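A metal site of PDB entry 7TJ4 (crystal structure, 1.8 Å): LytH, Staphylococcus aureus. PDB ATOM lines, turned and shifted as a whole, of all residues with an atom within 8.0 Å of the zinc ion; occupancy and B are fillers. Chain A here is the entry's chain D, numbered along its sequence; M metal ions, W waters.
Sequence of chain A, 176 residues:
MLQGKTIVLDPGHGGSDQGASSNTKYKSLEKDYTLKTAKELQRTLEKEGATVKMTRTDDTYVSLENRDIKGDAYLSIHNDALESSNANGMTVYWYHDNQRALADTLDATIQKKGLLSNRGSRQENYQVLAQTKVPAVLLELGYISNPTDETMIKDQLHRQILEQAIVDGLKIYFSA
OG of Ser 76 sits close to NE2 of His 78 (3.1 Å). The backbone NH of His 78 sits at hydrogen-bond distance from the backbone carbonyl oxygen of Leu 139, 2.8 Å away. The backbone NH (N) of Asn 79 lies close to the side-chain carboxylate (OE2) of Glu 30 (2.9 Å). The backbone NH (N) of Glu 30 is in hydrogen-bond range of the backbone carbonyl oxygen (O) of Ala 20 (2.8 Å). OG1 of Thr 34 lies close to O of Glu 30 (3.3 Å). ND1 of His 13 is in hydrogen-bond range of OD2 of Asp 17, 2.6 Å away. OE1 of Glu 140 lies close to N of Asn 79, 3.3 Å away.
Merely in contact with the zinc ion: Asn 79 (3.98 Å). The nearest printed residue that does not touch the zinc ion is Glu 140 (4.5 Å).
The zinc ion is bound by ND1 of His 78 (2.0 Å), water W1 (2.2 Å), OE2 of Glu 30 (2.2 Å), NE2 of His 13 (2.2 Å) and water W2 (2.4 Å).
Water W1 lies within hydrogen-bond range of OE2 of Glu 140 and O of Asn 79.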
ATOM      1  N   PRO A  11      11.075  20.577  11.276  1.00  0.00           N
ATOM      2  CA  PRO A  11      11.269  21.809  10.525  1.00  0.00           C
ATOM      3  C   PRO A  11      11.270  21.546   9.024  1.00  0.00           C
ATOM      4  O   PRO A  11      12.192  20.891   8.508  1.00  0.00           O
ATOM      5  CB  PRO A  11      12.618  22.333  11.038  1.00  0.00           C
ATOM      6  CG  PRO A  11      13.327  21.150  11.578  1.00  0.00           C
ATOM      7  CD  PRO A  11      12.294  20.096  11.929  1.00  0.00           C
ATOM      8  N   GLY A  12      10.247  22.019   8.308  1.00  0.00           N
ATOM      9  CA  GLY A  12      10.098  21.614   6.925  1.00  0.00           C
ATOM     10  C   GLY A  12      11.283  21.991   6.066  1.00  0.00           C
ATOM     11  O   GLY A  12      11.986  22.988   6.325  1.00  0.00           O
ATOM     12  N   HIS A  13      11.513  21.181   5.020  1.00  0.00           N
ATOM     13  CA  HIS A  13      12.536  21.433   4.006  1.00  0.00           C
ATOM     14  C   HIS A  13      13.958  21.322   4.587  1.00  0.00           C
ATOM     15  O   HIS A  13      14.120  20.769   5.681  1.00  0.00           O
ATOM     16  CB  HIS A  13      12.246  22.778   3.320  1.00  0.00           C
ATOM     17  CG  HIS A  13      10.812  22.896   2.913  1.00  0.00           C
ATOM     18  ND1 HIS A  13      10.315  22.255   1.796  1.00  0.00           N
ATOM     19  CD2 HIS A  13       9.751  23.480   3.519  1.00  0.00           C
ATOM     20  CE1 HIS A  13       9.016  22.483   1.701  1.00  0.00           C
ATOM     21  NE2 HIS A  13       8.636  23.204   2.743  1.00  0.00           N
ATOM     22  N   ASP A  17      16.383  21.407  -0.750  1.00  0.00           N
ATOM     23  CA  ASP A  17      14.982  21.841  -0.793  1.00  0.00           C
ATOM     24  C   ASP A  17      14.842  23.137   0.008  1.00  0.00           C
ATOM     25  O   ASP A  17      14.870  23.101   1.231  1.00  0.00           O
ATOM     26  CB  ASP A  17      14.077  20.757  -0.217  1.00  0.00           C
ATOM     27  CG  ASP A  17      12.607  21.193  -0.130  1.00  0.00           C
ATOM     28  OD1 ASP A  17      12.182  22.190  -0.808  1.00  0.00           O
ATOM     29  OD2 ASP A  17      11.872  20.545   0.628  1.00  0.00           O
ATOM     30  N   GLN A  18      14.684  24.270  -0.693  1.00  0.00           N
ATOM     31  CA  GLN A  18      14.618  25.561   0.026  1.00  0.00           C
ATOM     32  C   GLN A  18      13.256  25.856   0.632  1.00  0.00           C
ATOM     33  O   GLN A  18      13.151  26.757   1.492  1.00  0.00           O
ATOM     34  CB  GLN A  18      14.921  26.727  -0.891  1.00  0.00           C
ATOM     35  CG  GLN A  18      16.289  26.708  -1.445  1.00  0.00           C
ATOM     36  CD  GLN A  18      16.619  27.966  -2.174  1.00  0.00           C
ATOM     37  OE1 GLN A  18      15.730  28.659  -2.719  1.00  0.00           O
ATOM     38  NE2 GLN A  18      17.891  28.310  -2.169  1.00  0.00           N
ATOM     39  N   GLY A  19      12.210  25.157   0.174  1.00  0.00           N
ATOM     40  CA  GLY A  19      10.840  25.504   0.414  1.00  0.00           C
ATOM     41  C   GLY A  19      10.508  26.762  -0.349  1.00  0.00           C
ATOM     42  O   GLY A  19      11.115  27.094  -1.368  1.00  0.00           O
ATOM     43  N   ALA A  20       9.544  27.498   0.172  1.00  0.00           N
ATOM     44  CA  ALA A  20       9.139  28.745  -0.432  1.00  0.00           C
ATOM     45  C   ALA A  20      10.149  29.855  -0.112  1.00  0.00           C
ATOM     46  O   ALA A  20      10.820  29.844   0.931  1.00  0.00           O
ATOM     47  CB  ALA A  20       7.755  29.158   0.072  1.00  0.00           C
ATOM     48  N   GLU A  30      12.120  29.623   3.378  1.00  0.00           N
ATOM     49  CA  GLU A  30      11.359  28.839   4.347  1.00  0.00           C
ATOM     50  C   GLU A  30      12.250  27.874   5.119  1.00  0.00           C
ATOM     51  O   GLU A  30      12.103  27.746   6.336  1.00  0.00           O
ATOM     52  CB  GLU A  30      10.253  28.081   3.611  1.00  0.00           C
ATOM     53  CG  GLU A  30       9.457  27.181   4.510  1.00  0.00           C
ATOM     54  CD  GLU A  30       8.368  26.410   3.744  1.00  0.00           C
ATOM     55  OE1 GLU A  30       8.329  26.538   2.486  1.00  0.00           O
ATOM     56  OE2 GLU A  30       7.568  25.678   4.367  1.00  0.00           O
ATOM     57  N   LYS A  31      13.188  27.189   4.448  1.00  0.00           N
ATOM     58  CA  LYS A  31      13.957  26.163   5.145  1.00  0.00           C
ATOM     59  C   LYS A  31      14.773  26.772   6.279  1.00  0.00           C
ATOM     60  O   LYS A  31      15.094  26.077   7.254  1.00  0.00           O
ATOM     61  CB  LYS A  31      14.886  25.403   4.194  1.00  0.00           C
ATOM     62  CG  LYS A  31      15.992  26.237   3.522  1.00  0.00           C
ATOM     63  CD  LYS A  31      17.087  25.360   2.962  1.00  0.00           C
ATOM     64  CE  LYS A  31      18.115  26.189   2.235  1.00  0.00           C
ATOM     65  NZ  LYS A  31      19.362  25.404   1.943  1.00  0.00           N
ATOM     66  N   THR A  34      11.898  27.795   9.256  1.00  0.00           N
ATOM     67  CA  THR A  34      11.371  26.603   9.937  1.00  0.00           C
ATOM     68  C   THR A  34      12.401  26.050  10.914  1.00  0.00           C
ATOM     69  O   THR A  34      12.039  25.637  12.024  1.00  0.00           O
ATOM     70  CB  THR A  34      10.944  25.513   8.940  1.00  0.00           C
ATOM     71  OG1 THR A  34      12.079  25.060   8.217  1.00  0.00           O
ATOM     72  CG2 THR A  34       9.901  26.007   7.948  1.00  0.00           C
ATOM     73  N   SER A  76       4.991  19.521  12.551  1.00  0.00           N
ATOM     74  CA  SER A  76       5.715  19.963  11.360  1.00  0.00           C
ATOM     75  C   SER A  76       5.584  21.467  11.217  1.00  0.00           C
ATOM     76  O   SER A  76       4.490  22.032  11.360  1.00  0.00           O
ATOM     77  CB  SER A  76       5.185  19.252  10.107  1.00  0.00           C
ATOM     78  OG  SER A  76       6.042  19.524   9.024  1.00  0.00           O
ATOM     79  N   ILE A  77       6.689  22.127  10.922  1.00  0.00           N
ATOM     80  CA  ILE A  77       6.715  23.583  10.929  1.00  0.00           C
ATOM     81  C   ILE A  77       7.055  24.033   9.536  1.00  0.00           C
ATOM     82  O   ILE A  77       8.079  23.638   8.975  1.00  0.00           O
ATOM     83  CB  ILE A  77       7.736  24.091  11.972  1.00  0.00           C
ATOM     84  CG1 ILE A  77       7.323  23.513  13.318  1.00  0.00           C
ATOM     85  CG2 ILE A  77       7.836  25.645  11.946  1.00  0.00           C
ATOM     86  CD1 ILE A  77       8.498  23.368  14.277  1.00  0.00           C
ATOM     87  N   HIS A  78       6.191  24.884   8.987  1.00  0.00           N
ATOM     88  CA  HIS A  78       6.305  25.348   7.620  1.00  0.00           C
ATOM     89  C   HIS A  78       5.945  26.830   7.525  1.00  0.00           C
ATOM     90  O   HIS A  78       5.479  27.461   8.478  1.00  0.00           O
ATOM     91  CB  HIS A  78       5.409  24.508   6.707  1.00  0.00           C
ATOM     92  CG  HIS A  78       5.966  23.165   6.388  1.00  0.00           C
ATOM     93  ND1 HIS A  78       6.526  22.854   5.168  1.00  0.00           N
ATOM     94  CD2 HIS A  78       6.026  22.031   7.130  1.00  0.00           C
ATOM     95  CE1 HIS A  78       6.904  21.585   5.158  1.00  0.00           C
ATOM     96  NE2 HIS A  78       6.614  21.064   6.340  1.00  0.00           N
ATOM     97  N   ASN A  79       6.195  27.382   6.331  1.00  0.00           N
ATOM     98  CA  ASN A  79       5.661  28.655   5.892  1.00  0.00           C
ATOM     99  C   ASN A  79       4.987  28.489   4.537  1.00  0.00           C
ATOM    100  O   ASN A  79       5.416  27.689   3.708  1.00  0.00           O
ATOM    101  CB  ASN A  79       6.721  29.725   5.786  1.00  0.00           C
ATOM    102  CG  ASN A  79       7.375  29.986   7.105  1.00  0.00           C
ATOM    103  OD1 ASN A  79       8.462  29.450   7.383  1.00  0.00           O
ATOM    104  ND2 ASN A  79       6.724  30.803   7.952  1.00  0.00           N
ATOM    105  N   ASP A  80       3.931  29.263   4.346  1.00  0.00           N
ATOM    106  CA  ASP A  80       3.073  29.197   3.188  1.00  0.00           C
ATOM    107  C   ASP A  80       3.597  30.079   2.066  1.00  0.00           C
ATOM    108  O   ASP A  80       4.424  31.005   2.272  1.00  0.00           O
ATOM    109  CB  ASP A  80       1.646  29.594   3.593  1.00  0.00           C
ATOM    110  CG  ASP A  80       0.632  28.427   3.429  1.00  0.00           C
ATOM    111  OD1 ASP A  80       0.968  27.480   2.712  1.00  0.00           O
ATOM    112  OD2 ASP A  80      -0.489  28.449   4.022  1.00  0.00           O
ATOM    113  N   ALA A  81       3.169  29.752   0.846  1.00  0.00           N
ATOM    114  CA  ALA A  81       3.432  30.577  -0.317  1.00  0.00           C
ATOM    115  C   ALA A  81       2.274  30.498  -1.285  1.00  0.00           C
ATOM    116  O   ALA A  81       1.606  29.455  -1.410  1.00  0.00           O
ATOM    117  CB  ALA A  81       4.709  30.188  -1.049  1.00  0.00           C
ATOM    118  N   TYR A 126      -1.001  15.806   3.978  1.00  0.00           N
ATOM    119  CA  TYR A 126       0.439  15.927   3.854  1.00  0.00           C
ATOM    120  C   TYR A 126       1.012  14.590   4.256  1.00  0.00           C
ATOM    121  O   TYR A 126       0.627  14.035   5.293  1.00  0.00           O
ATOM    122  CB  TYR A 126       1.025  17.004   4.754  1.00  0.00           C
ATOM    123  CG  TYR A 126       0.593  18.388   4.420  1.00  0.00           C
ATOM    124  CD1 TYR A 126      -0.614  18.868   4.888  1.00  0.00           C
ATOM    125  CD2 TYR A 126       1.427  19.245   3.716  1.00  0.00           C
ATOM    126  CE1 TYR A 126      -1.018  20.141   4.614  1.00  0.00           C
ATOM    127  CE2 TYR A 126       1.036  20.517   3.436  1.00  0.00           C
ATOM    128  CZ  TYR A 126      -0.185  20.954   3.882  1.00  0.00           C
ATOM    129  OH  TYR A 126      -0.605  22.210   3.629  1.00  0.00           O
ATOM    130  N   LEU A 138       0.500  19.988  11.031  1.00  0.00           N
ATOM    131  CA  LEU A 138       1.442  20.796  10.285  1.00  0.00           C
ATOM    132  C   LEU A 138       1.055  22.246  10.448  1.00  0.00           C
ATOM    133  O   LEU A 138      -0.079  22.642  10.132  1.00  0.00           O
ATOM    134  CB  LEU A 138       1.495  20.381   8.817  1.00  0.00           C
ATOM    135  CG  LEU A 138       2.610  20.974   7.971  1.00  0.00           C
ATOM    136  CD1 LEU A 138       2.989  19.927   6.923  1.00  0.00           C
ATOM    137  CD2 LEU A 138       2.146  22.241   7.295  1.00  0.00           C
ATOM    138  N   LEU A 139       2.012  23.056  10.885  1.00  0.00           N
ATOM    139  CA  LEU A 139       1.778  24.466  11.188  1.00  0.00           C
ATOM    140  C   LEU A 139       2.303  25.318  10.056  1.00  0.00           C
ATOM    141  O   LEU A 139       3.489  25.257   9.721  1.00  0.00           O
ATOM    142  CB  LEU A 139       2.475  24.816  12.512  1.00  0.00           C
ATOM    143  CG  LEU A 139       1.822  24.058  13.679  1.00  0.00           C
ATOM    144  CD1 LEU A 139       2.841  23.764  14.728  1.00  0.00           C
ATOM    145  CD2 LEU A 139       0.727  24.899  14.285  1.00  0.00           C
ATOM    146  N   GLU A 140       1.426  26.057   9.415  1.00  0.00           N
ATOM    147  CA  GLU A 140       1.878  27.063   8.439  1.00  0.00           C
ATOM    148  C   GLU A 140       1.941  28.409   9.175  1.00  0.00           C
ATOM    149  O   GLU A 140       0.915  29.079   9.344  1.00  0.00           O
ATOM    150  CB  GLU A 140       0.965  27.096   7.215  1.00  0.00           C
ATOM    151  CG  GLU A 140       0.970  25.850   6.336  1.00  0.00           C
ATOM    152  CD  GLU A 140       2.252  25.716   5.494  1.00  0.00           C
ATOM    153  OE1 GLU A 140       3.105  26.651   5.574  1.00  0.00           O
ATOM    154  OE2 GLU A 140       2.379  24.681   4.741  1.00  0.00           O
HETATM  155 ZN    ZN M   1       6.647  23.914   3.418  1.00  0.00          ZN
HETATM  156  O   HOH W   1       4.678  24.892   3.366  1.00  0.00           O
HETATM  157  O   HOH W   2       6.631  24.934   1.201  1.00  0.00           O
